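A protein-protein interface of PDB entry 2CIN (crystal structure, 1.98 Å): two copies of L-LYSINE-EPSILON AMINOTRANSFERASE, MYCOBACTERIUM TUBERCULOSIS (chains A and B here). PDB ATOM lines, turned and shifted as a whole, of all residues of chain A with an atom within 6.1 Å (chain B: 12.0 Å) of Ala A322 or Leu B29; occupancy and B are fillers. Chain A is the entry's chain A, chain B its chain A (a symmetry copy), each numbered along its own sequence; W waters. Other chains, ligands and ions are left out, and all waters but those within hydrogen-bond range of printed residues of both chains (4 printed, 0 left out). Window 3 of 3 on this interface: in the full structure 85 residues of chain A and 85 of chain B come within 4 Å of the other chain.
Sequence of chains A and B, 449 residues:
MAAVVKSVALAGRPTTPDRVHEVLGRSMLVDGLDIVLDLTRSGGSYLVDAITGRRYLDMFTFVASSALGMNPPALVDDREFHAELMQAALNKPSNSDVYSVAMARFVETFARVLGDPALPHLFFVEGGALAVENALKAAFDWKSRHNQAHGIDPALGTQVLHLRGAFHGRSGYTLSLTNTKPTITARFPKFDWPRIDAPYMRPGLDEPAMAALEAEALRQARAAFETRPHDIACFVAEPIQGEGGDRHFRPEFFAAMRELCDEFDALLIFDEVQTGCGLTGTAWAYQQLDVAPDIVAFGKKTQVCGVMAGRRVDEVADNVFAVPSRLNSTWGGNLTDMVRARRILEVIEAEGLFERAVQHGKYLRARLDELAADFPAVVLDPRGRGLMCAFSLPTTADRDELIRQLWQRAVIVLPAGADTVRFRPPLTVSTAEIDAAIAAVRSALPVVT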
ATOM      1  N   TYR A  99      -4.068 -11.835  12.285  1.00  0.00           N
ATOM      2  CA  TYR A  99      -2.863 -12.426  12.871  1.00  0.00           C
ATOM      3  C   TYR A  99      -1.967 -13.039  11.813  1.00  0.00           C
ATOM      4  O   TYR A  99      -2.438 -13.403  10.741  1.00  0.00           O
ATOM      5  CB  TYR A  99      -3.241 -13.459  13.941  1.00  0.00           C
ATOM      6  CG  TYR A  99      -4.211 -12.888  14.951  1.00  0.00           C
ATOM      7  CD1 TYR A  99      -4.020 -11.611  15.503  1.00  0.00           C
ATOM      8  CD2 TYR A  99      -5.341 -13.606  15.337  1.00  0.00           C
ATOM      9  CE1 TYR A  99      -4.928 -11.068  16.416  1.00  0.00           C
ATOM     10  CE2 TYR A  99      -6.253 -13.067  16.245  1.00  0.00           C
ATOM     11  CZ  TYR A  99      -6.033 -11.814  16.783  1.00  0.00           C
ATOM     12  OH  TYR A  99      -6.950 -11.317  17.679  1.00  0.00           O
ATOM     13  N   LEU A 122      -0.105  -9.062  27.565  1.00  0.00           N
ATOM     14  CA  LEU A 122       0.656  -8.192  26.678  1.00  0.00           C
ATOM     15  C   LEU A 122      -0.312  -7.417  25.789  1.00  0.00           C
ATOM     16  O   LEU A 122      -1.343  -7.962  25.364  1.00  0.00           O
ATOM     17  CB  LEU A 122       1.595  -9.051  25.839  1.00  0.00           C
ATOM     18  CG  LEU A 122       3.045  -9.294  26.291  1.00  0.00           C
ATOM     19  CD1 LEU A 122       3.388  -9.019  27.735  1.00  0.00           C
ATOM     20  CD2 LEU A 122       3.627 -10.578  25.786  1.00  0.00           C
ATOM     21  N   VAL A 316      -9.669  -8.488  39.178  1.00  0.00           N
ATOM     22  CA  VAL A 316     -10.920  -7.961  38.605  1.00  0.00           C
ATOM     23  C   VAL A 316     -11.079  -8.789  37.332  1.00  0.00           C
ATOM     24  O   VAL A 316     -10.327  -8.600  36.367  1.00  0.00           O
ATOM     25  CB  VAL A 316     -10.837  -6.408  38.334  1.00  0.00           C
ATOM     26  CG1 VAL A 316     -11.910  -5.919  37.348  1.00  0.00           C
ATOM     27  CG2 VAL A 316     -10.892  -5.610  39.650  1.00  0.00           C
ATOM     28  N   ALA A 317     -12.015  -9.740  37.351  1.00  0.00           N
ATOM     29  CA  ALA A 317     -12.118 -10.729  36.276  1.00  0.00           C
ATOM     30  C   ALA A 317     -12.490 -10.109  34.916  1.00  0.00           C
ATOM     31  O   ALA A 317     -12.124 -10.665  33.894  1.00  0.00           O
ATOM     32  CB  ALA A 317     -13.093 -11.871  36.643  1.00  0.00           C
ATOM     33  N   ASP A 318     -13.221  -8.987  34.923  1.00  0.00           N
ATOM     34  CA  ASP A 318     -13.669  -8.356  33.668  1.00  0.00           C
ATOM     35  C   ASP A 318     -12.818  -7.108  33.371  1.00  0.00           C
ATOM     36  O   ASP A 318     -13.313  -6.096  32.918  1.00  0.00           O
ATOM     37  CB  ASP A 318     -15.189  -8.076  33.663  1.00  0.00           C
ATOM     38  CG  ASP A 318     -15.716  -7.519  35.009  1.00  0.00           C
ATOM     39  OD1 ASP A 318     -14.943  -7.388  35.982  1.00  0.00           O
ATOM     40  OD2 ASP A 318     -16.928  -7.229  35.104  1.00  0.00           O
ATOM     41  N   ASN A 319     -11.525  -7.215  33.640  1.00  0.00           N
ATOM     42  CA  ASN A 319     -10.560  -6.169  33.335  1.00  0.00           C
ATOM     43  C   ASN A 319     -10.372  -6.028  31.791  1.00  0.00           C
ATOM     44  O   ASN A 319     -10.904  -6.797  30.985  1.00  0.00           O
ATOM     45  CB  ASN A 319      -9.224  -6.453  34.059  1.00  0.00           C
ATOM     46  CG  ASN A 319      -8.491  -7.671  33.497  1.00  0.00           C
ATOM     47  OD1 ASN A 319      -8.021  -7.647  32.358  1.00  0.00           O
ATOM     48  ND2 ASN A 319      -8.417  -8.751  34.270  1.00  0.00           N
ATOM     49  N   VAL A 320      -9.562  -5.058  31.410  1.00  0.00           N
ATOM     50  CA  VAL A 320      -9.481  -4.543  30.048  1.00  0.00           C
ATOM     51  C   VAL A 320      -8.745  -5.576  29.158  1.00  0.00           C
ATOM     52  O   VAL A 320      -8.874  -5.565  27.927  1.00  0.00           O
ATOM     53  CB  VAL A 320      -8.851  -3.139  30.236  1.00  0.00           C
ATOM     54  CG1 VAL A 320      -7.369  -3.061  29.979  1.00  0.00           C
ATOM     55  CG2 VAL A 320      -9.765  -1.984  29.934  1.00  0.00           C
ATOM     56  N   PHE A 321      -8.034  -6.511  29.781  1.00  0.00           N
ATOM     57  CA  PHE A 321      -7.334  -7.576  29.047  1.00  0.00           C
ATOM     58  C   PHE A 321      -8.185  -8.822  28.825  1.00  0.00           C
ATOM     59  O   PHE A 321      -7.780  -9.738  28.114  1.00  0.00           O
ATOM     60  CB  PHE A 321      -6.017  -7.918  29.742  1.00  0.00           C
ATOM     61  CG  PHE A 321      -5.152  -6.705  29.964  1.00  0.00           C
ATOM     62  CD1 PHE A 321      -4.431  -6.158  28.905  1.00  0.00           C
ATOM     63  CD2 PHE A 321      -5.099  -6.087  31.206  1.00  0.00           C
ATOM     64  CE1 PHE A 321      -3.657  -5.010  29.090  1.00  0.00           C
ATOM     65  CE2 PHE A 321      -4.335  -4.934  31.411  1.00  0.00           C
ATOM     66  CZ  PHE A 321      -3.617  -4.392  30.337  1.00  0.00           C
ATOM     67  N   ALA A 322      -9.367  -8.839  29.427  1.00  0.00           N
ATOM     68  CA  ALA A 322     -10.238  -9.992  29.414  1.00  0.00           C
ATOM     69  C   ALA A 322     -11.498  -9.710  28.605  1.00  0.00           C
ATOM     70  O   ALA A 322     -12.163 -10.630  28.175  1.00  0.00           O
ATOM     71  CB  ALA A 322     -10.598 -10.356  30.854  1.00  0.00           C
ATOM     72  N   VAL A 323     -11.813  -8.430  28.391  1.00  0.00           N
ATOM     73  CA  VAL A 323     -13.063  -7.980  27.779  1.00  0.00           C
ATOM     74  C   VAL A 323     -12.691  -7.377  26.421  1.00  0.00           C
ATOM     75  O   VAL A 323     -11.833  -6.489  26.366  1.00  0.00           O
ATOM     76  CB  VAL A 323     -13.762  -6.911  28.669  1.00  0.00           C
ATOM     77  CG1 VAL A 323     -14.992  -6.264  27.974  1.00  0.00           C
ATOM     78  CG2 VAL A 323     -14.171  -7.540  30.006  1.00  0.00           C
ATOM     79  N   PRO A 324     -13.327  -7.854  25.337  1.00  0.00           N
ATOM     80  CA  PRO A 324     -13.041  -7.347  23.983  1.00  0.00           C
ATOM     81  C   PRO A 324     -13.348  -5.854  23.822  1.00  0.00           C
ATOM     82  O   PRO A 324     -14.289  -5.330  24.435  1.00  0.00           O
ATOM     83  CB  PRO A 324     -13.997  -8.150  23.074  1.00  0.00           C
ATOM     84  CG  PRO A 324     -14.478  -9.254  23.863  1.00  0.00           C
ATOM     85  CD  PRO A 324     -14.387  -8.880  25.328  1.00  0.00           C
ATOM     86  N   SER A 325     -12.508  -5.186  23.025  1.00  0.00           N
ATOM     87  CA  SER A 325     -12.762  -3.829  22.532  1.00  0.00           C
ATOM     88  C   SER A 325     -12.628  -2.718  23.562  1.00  0.00           C
ATOM     89  O   SER A 325     -13.010  -1.590  23.284  1.00  0.00           O
ATOM     90  CB  SER A 325     -14.114  -3.740  21.792  1.00  0.00           C
ATOM     91  OG  SER A 325     -13.982  -2.926  20.612  1.00  0.00           O
ATOM     92  N   VAL B  20      -0.561 -20.267  15.500  1.00  0.00           N
ATOM     93  CA  VAL B  20      -0.560 -18.817  15.722  1.00  0.00           C
ATOM     94  C   VAL B  20      -1.553 -18.375  16.814  1.00  0.00           C
ATOM     95  O   VAL B  20      -1.162 -17.674  17.755  1.00  0.00           O
ATOM     96  CB  VAL B  20      -0.811 -18.048  14.404  1.00  0.00           C
ATOM     97  CG1 VAL B  20      -1.269 -16.594  14.680  1.00  0.00           C
ATOM     98  CG2 VAL B  20       0.426 -18.128  13.516  1.00  0.00           C
ATOM     99  N   HIS B  21      -2.816 -18.786  16.694  1.00  0.00           N
ATOM    100  CA  HIS B  21      -3.851 -18.411  17.662  1.00  0.00           C
ATOM    101  C   HIS B  21      -3.559 -18.924  19.078  1.00  0.00           C
ATOM    102  O   HIS B  21      -3.827 -18.219  20.052  1.00  0.00           O
ATOM    103  CB  HIS B  21      -5.259 -18.840  17.215  1.00  0.00           C
ATOM    104  CG  HIS B  21      -5.746 -18.125  15.997  1.00  0.00           C
ATOM    105  ND1 HIS B  21      -6.761 -17.189  16.036  1.00  0.00           N
ATOM    106  CD2 HIS B  21      -5.346 -18.194  14.703  1.00  0.00           C
ATOM    107  CE1 HIS B  21      -6.982 -16.734  14.814  1.00  0.00           C
ATOM    108  NE2 HIS B  21      -6.132 -17.324  13.989  1.00  0.00           N
ATOM    109  N   GLU B  22      -2.985 -20.118  19.162  1.00  0.00           N
ATOM    110  CA  GLU B  22      -2.601 -20.711  20.431  1.00  0.00           C
ATOM    111  C   GLU B  22      -1.484 -19.889  21.108  1.00  0.00           C
ATOM    112  O   GLU B  22      -1.619 -19.539  22.269  1.00  0.00           O
ATOM    113  CB  GLU B  22      -2.158 -22.170  20.230  1.00  0.00           C
ATOM    114  CG  GLU B  22      -1.550 -22.784  21.490  1.00  0.00           C
ATOM    115  CD  GLU B  22      -0.793 -24.097  21.241  1.00  0.00           C
ATOM    116  OE1 GLU B  22      -1.004 -24.724  20.169  1.00  0.00           O
ATOM    117  OE2 GLU B  22       0.002 -24.495  22.141  1.00  0.00           O
ATOM    118  N   VAL B  23      -0.406 -19.597  20.369  1.00  0.00           N
ATOM    119  CA  VAL B  23       0.743 -18.817  20.851  1.00  0.00           C
ATOM    120  C   VAL B  23       0.294 -17.428  21.312  1.00  0.00           C
ATOM    121  O   VAL B  23       0.608 -17.001  22.418  1.00  0.00           O
ATOM    122  CB  VAL B  23       1.913 -18.728  19.796  1.00  0.00           C
ATOM    123  CG1 VAL B  23       2.989 -17.756  20.247  1.00  0.00           C
ATOM    124  CG2 VAL B  23       2.563 -20.108  19.543  1.00  0.00           C
ATOM    125  N   LEU B  24      -0.487 -16.739  20.486  1.00  0.00           N
ATOM    126  CA  LEU B  24      -0.962 -15.409  20.848  1.00  0.00           C
ATOM    127  C   LEU B  24      -1.901 -15.436  22.041  1.00  0.00           C
ATOM    128  O   LEU B  24      -1.881 -14.502  22.842  1.00  0.00           O
ATOM    129  CB  LEU B  24      -1.673 -14.734  19.657  1.00  0.00           C
ATOM    130  CG  LEU B  24      -0.788 -14.384  18.437  1.00  0.00           C
ATOM    131  CD1 LEU B  24      -1.662 -13.841  17.304  1.00  0.00           C
ATOM    132  CD2 LEU B  24       0.300 -13.403  18.792  1.00  0.00           C
ATOM    133  N   GLY B  25      -2.761 -16.459  22.116  1.00  0.00           N
ATOM    134  CA  GLY B  25      -3.758 -16.592  23.203  1.00  0.00           C
ATOM    135  C   GLY B  25      -3.158 -16.743  24.597  1.00  0.00           C
ATOM    136  O   GLY B  25      -3.809 -16.428  25.583  1.00  0.00           O
ATOM    137  N   ARG B  26      -1.910 -17.183  24.687  1.00  0.00           N
ATOM    138  CA  ARG B  26      -1.187 -17.169  25.975  1.00  0.00           C
ATOM    139  C   ARG B  26      -0.891 -15.745  26.537  1.00  0.00           C
ATOM    140  O   ARG B  26      -0.657 -15.590  27.743  1.00  0.00           O
ATOM    141  CB  ARG B  26       0.141 -17.934  25.854  1.00  0.00           C
ATOM    142  CG  ARG B  26       0.044 -19.428  25.490  1.00  0.00           C
ATOM    143  CD  ARG B  26       1.481 -19.929  25.301  1.00  0.00           C
ATOM    144  NE  ARG B  26       1.644 -21.005  24.309  1.00  0.00           N
ATOM    145  CZ  ARG B  26       2.741 -21.182  23.558  1.00  0.00           C
ATOM    146  NH1 ARG B  26       3.780 -20.339  23.640  1.00  0.00           N
ATOM    147  NH2 ARG B  26       2.795 -22.194  22.698  1.00  0.00           N
ATOM    148  N   SER B  27      -0.875 -14.729  25.665  1.00  0.00           N
ATOM    149  CA  SER B  27      -0.462 -13.374  26.048  1.00  0.00           C
ATOM    150  C   SER B  27      -1.541 -12.306  25.847  1.00  0.00           C
ATOM    151  O   SER B  27      -1.495 -11.254  26.472  1.00  0.00           O
ATOM    152  CB  SER B  27       0.791 -12.965  25.256  1.00  0.00           C
ATOM    153  OG  SER B  27       1.855 -13.829  25.531  1.00  0.00           O
ATOM    154  N   MET B  28      -2.504 -12.575  24.966  1.00  0.00           N
ATOM    155  CA  MET B  28      -3.454 -11.559  24.561  1.00  0.00           C
ATOM    156  C   MET B  28      -4.820 -12.156  24.378  1.00  0.00           C
ATOM    157  O   MET B  28      -4.975 -13.355  24.185  1.00  0.00           O
ATOM    158  CB  MET B  28      -3.057 -10.934  23.209  1.00  0.00           C
ATOM    159  CG  MET B  28      -1.562 -10.869  22.910  1.00  0.00           C
ATOM    160  SD  MET B  28      -1.175 -10.069  21.312  1.00  0.00           S
ATOM    161  CE  MET B  28      -2.746 -10.176  20.511  1.00  0.00           C
ATOM    162  N   LEU B  29      -5.802 -11.277  24.406  1.00  0.00           N
ATOM    163  CA  LEU B  29      -7.140 -11.574  23.985  1.00  0.00           C
ATOM    164  C   LEU B  29      -7.174 -11.746  22.455  1.00  0.00           C
ATOM    165  O   LEU B  29      -6.824 -10.823  21.718  1.00  0.00           O
ATOM    166  CB  LEU B  29      -8.031 -10.401  24.421  1.00  0.00           C
ATOM    167  CG  LEU B  29      -9.525 -10.661  24.536  1.00  0.00           C
ATOM    168  CD1 LEU B  29      -9.733 -11.716  25.597  1.00  0.00           C
ATOM    169  CD2 LEU B  29     -10.184  -9.378  24.917  1.00  0.00           C
ATOM    170  N   VAL B  30      -7.573 -12.913  21.969  1.00  0.00           N
ATOM    171  CA  VAL B  30      -7.506 -13.162  20.526  1.00  0.00           C
ATOM    172  C   VAL B  30      -8.904 -13.127  19.865  1.00  0.00           C
ATOM    173  O   VAL B  30      -9.478 -14.161  19.530  1.00  0.00           O
ATOM    174  CB  VAL B  30      -6.632 -14.435  20.146  1.00  0.00           C
ATOM    175  CG1 VAL B  30      -6.712 -15.507  21.194  1.00  0.00           C
ATOM    176  CG2 VAL B  30      -7.049 -15.025  18.819  1.00  0.00           C
ATOM    177  N   ASP B  31      -9.445 -11.934  19.668  1.00  0.00           N
ATOM    178  CA  ASP B  31     -10.800 -11.829  19.135  1.00  0.00           C
ATOM    179  C   ASP B  31     -10.867 -11.454  17.636  1.00  0.00           C
ATOM    180  O   ASP B  31     -11.939 -11.107  17.149  1.00  0.00           O
ATOM    181  CB  ASP B  31     -11.614 -10.839  19.970  1.00  0.00           C
ATOM    182  CG  ASP B  31     -11.016  -9.438  19.958  1.00  0.00           C
ATOM    183  OD1 ASP B  31      -9.756  -9.311  19.928  1.00  0.00           O
ATOM    184  OD2 ASP B  31     -11.814  -8.461  19.961  1.00  0.00           O
ATOM    185  N   GLY B  32      -9.751 -11.537  16.913  1.00  0.00           N
ATOM    186  CA  GLY B  32      -9.754 -11.168  15.502  1.00  0.00           C
ATOM    187  C   GLY B  32     -10.301 -12.248  14.577  1.00  0.00           C
ATOM    188  O   GLY B  32     -11.006 -13.161  15.014  1.00  0.00           O
ATOM    189  N   LEU B  33      -9.965 -12.147  13.297  1.00  0.00           N
ATOM    190  CA  LEU B  33     -10.441 -13.081  12.273  1.00  0.00           C
ATOM    191  C   LEU B  33      -9.886 -14.499  12.444  1.00  0.00           C
ATOM    192  O   LEU B  33      -8.772 -14.695  12.972  1.00  0.00           O
ATOM    193  CB  LEU B  33     -10.131 -12.550  10.869  1.00  0.00           C
ATOM    194  CG  LEU B  33     -10.663 -11.169  10.500  1.00  0.00           C
ATOM    195  CD1 LEU B  33     -10.258 -10.795   9.079  1.00  0.00           C
ATOM    196  CD2 LEU B  33     -12.161 -11.148  10.636  1.00  0.00           C
ATOM    197  N   ASP B  34     -10.669 -15.477  11.986  1.00  0.00           N
ATOM    198  CA  ASP B  34     -10.299 -16.903  12.077  1.00  0.00           C
ATOM    199  C   ASP B  34      -9.090 -17.321  11.247  1.00  0.00           C
ATOM    200  O   ASP B  34      -8.542 -18.443  11.428  1.00  0.00           O
ATOM    201  CB  ASP B  34     -11.455 -17.792  11.631  1.00  0.00           C
ATOM    202  CG  ASP B  34     -12.329 -18.187  12.757  1.00  0.00           C
ATOM    203  OD1 ASP B  34     -12.018 -17.821  13.927  1.00  0.00           O
ATOM    204  OD2 ASP B  34     -13.344 -18.866  12.469  1.00  0.00           O
ATOM    205  N   ILE B  35      -8.661 -16.449  10.354  1.00  0.00           N
ATOM    206  CA  ILE B  35      -7.612 -16.827   9.439  1.00  0.00           C
ATOM    207  C   ILE B  35      -6.237 -16.468   9.971  1.00  0.00           C
ATOM    208  O   ILE B  35      -6.116 -15.756  10.983  1.00  0.00           O
ATOM    209  CB  ILE B  35      -7.846 -16.207   8.048  1.00  0.00           C
ATOM    210  CG1 ILE B  35      -7.826 -14.675   8.132  1.00  0.00           C
ATOM    211  CG2 ILE B  35      -9.186 -16.743   7.457  1.00  0.00           C
ATOM    212  CD1 ILE B  35      -7.486 -14.026   6.812  1.00  0.00           C
ATOM    213  N   ARG B 170      -9.052   6.593  20.467  1.00  0.00           N
ATOM    214  CA  ARG B 170      -9.149   6.029  21.805  1.00  0.00           C
ATOM    215  C   ARG B 170      -8.074   6.551  22.778  1.00  0.00           C
ATOM    216  O   ARG B 170      -7.746   5.915  23.796  1.00  0.00           O
ATOM    217  CB  ARG B 170      -9.064   4.507  21.684  1.00  0.00           C
ATOM    218  CG  ARG B 170     -10.299   3.870  21.013  1.00  0.00           C
ATOM    219  CD  ARG B 170      -9.963   2.385  20.905  1.00  0.00           C
ATOM    220  NE  ARG B 170     -10.960   1.570  20.239  1.00  0.00           N
ATOM    221  CZ  ARG B 170     -11.751   0.703  20.882  1.00  0.00           C
ATOM    222  NH1 ARG B 170     -11.690   0.583  22.204  1.00  0.00           N
ATOM    223  NH2 ARG B 170     -12.591  -0.054  20.194  1.00  0.00           N
ATOM    224  N   THR B 183     -18.723   0.732  25.178  1.00  0.00           N
ATOM    225  CA  THR B 183     -17.514  -0.067  25.412  1.00  0.00           C
ATOM    226  C   THR B 183     -16.210   0.733  25.193  1.00  0.00           C
ATOM    227  O   THR B 183     -15.218   0.538  25.888  1.00  0.00           O
ATOM    228  CB  THR B 183     -17.539  -1.306  24.464  1.00  0.00           C
ATOM    229  OG1 THR B 183     -18.646  -2.119  24.849  1.00  0.00           O
ATOM    230  CG2 THR B 183     -16.275  -2.143  24.558  1.00  0.00           C
ATOM    231  N   PHE B 188     -13.531   5.713  31.606  1.00  0.00           N
ATOM    232  CA  PHE B 188     -12.325   6.510  31.283  1.00  0.00           C
ATOM    233  C   PHE B 188     -12.626   8.003  31.534  1.00  0.00           C
ATOM    234  O   PHE B 188     -13.674   8.487  31.103  1.00  0.00           O
ATOM    235  CB  PHE B 188     -11.895   6.233  29.822  1.00  0.00           C
ATOM    236  CG  PHE B 188     -11.594   4.760  29.546  1.00  0.00           C
ATOM    237  CD1 PHE B 188     -10.830   4.008  30.462  1.00  0.00           C
ATOM    238  CD2 PHE B 188     -12.082   4.124  28.408  1.00  0.00           C
ATOM    239  CE1 PHE B 188     -10.563   2.647  30.247  1.00  0.00           C
ATOM    240  CE2 PHE B 188     -11.811   2.755  28.179  1.00  0.00           C
ATOM    241  CZ  PHE B 188     -11.035   2.023  29.094  1.00  0.00           C
HETATM  242  O   HOH W   1      -3.548  -8.867  26.982  1.00  0.00           O
HETATM  243  O   HOH W   2      -6.437 -13.365  12.021  1.00  0.00           O
HETATM  244  O   HOH W   3     -10.410  -6.334  21.642  1.00  0.00           O
HETATM  245  O   HOH W   4      -6.447  -9.338  18.978  1.00  0.00           O
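The side-chain hydroxyl (OH) of Tyr A99 lies within hydrogen-bond range of the backbone NH (N) of Asp B31. The side-chain hydroxyl of Tyr A99 lies within hydrogen-bond range of the backbone NH of Gly B32 (2.9 Å). O of Ser B27 lies within hydrogen-bond range of N of Leu A122 (2.8 Å). The backbone carbonyl oxygen (O) of Ser A325 is in hydrogen-bond range of the guanidinium group (NH1) of Arg B170 (2.8 Å).
N of Phe A321 sits at hydrogen-bond distance from OD1 of Asn A319, 2.8 Å away. OD1 of Asn A319 sits at hydrogen-bond distance from N of Ala A322 (3.4 Å). O of Ile B35 lies within hydrogen-bond range of NE2 of His B21, 3.4 Å away.
CE1 of His B21 touches CD2 of Tyr A99, at 3.6 Å. Leu B24 touches Tyr A99 (CD1 to CG, 3.6 Å). Tyr A99 touches Val B30 (CE2 to CG2, 3.3 Å). CD1 of Leu B29 touches O of Phe A321, at 3.7 Å. O of Ala A322 touches CD1 of Leu B29, 3.7 Å away. Val A323 touches Leu B29. N of Pro A324 touches CD2 of Leu B29, at 3.5 Å. Asp B31 touches Pro A324 (OD2 to CB, 3.8 Å). Pro A324 touches Thr B183. Ser A325 touches Thr B183.
Ala A322 touches one residue of chain B. Of chain A, only Phe A321, Ala A322, Val A323 and Pro A324 come within 4 Å of Leu B29. No residue of chain B comes within 4 Å of Ala A317. No residue of chain B comes within 4 Å of Asn A319. No residue of chain B comes within 4 Å of Val A320. Phe A321 touches just one residue of chain B: Leu B29. Val A323 touches one residue of chain B. Printed residues of chain A within 4 Å of His B21: Tyr A99. Of the printed residues of chain A, Leu B24 touches Tyr A99 (3.6 Å). Printed residues of chain A within 4 Å of Ser B27: Leu A122 (2.8 Å). Of the printed residues of chain A, Arg B170 touches Ser A325 (2.8 Å). Of the printed residues of chain A, Met B28 touches Leu A122. Val B23 touches none of the printed residues of chain A.
Hydrophobic or aromatic side chains of chain B that line the printed part of chain A: Val B20, His B21, Leu B24, Met B28, Leu B29 and Val B30. Among the printed residues, 16 pairs touch across the chains. Among the printed residues, no Asp or Glu carboxylate lies within 4 Å of a Lys or Arg side-chain nitrogen of the other chain.
No position is printed for both chains. Of the 16 pairs that touch across the chains among the printed residues, none has its exchanged pair printed and touching as well.
Water W4 lies within hydrogen-bond range of OH of Tyr A99 (2.4 Å), O of Leu B29 (3.1 Å) and OD1 of Asp B31 (3.4 Å). Water W2 lies within hydrogen-bond range of O of Ile B35 (2.6 Å), N of Tyr A99 (2.8 Å) and O of Leu B33 (2.9 Å). Water W3 bridges the backbone NH (N) of Ser A325 (2.8 Å) and the side-chain carboxylate (OD2) of Asp B31 (3.1 Å). Water W1 lies within hydrogen-bond range of the backbone carbonyl oxygen of Leu A122 (2.9 Å) and the backbone carbonyl oxygen of Ser B27 (3.2 Å).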
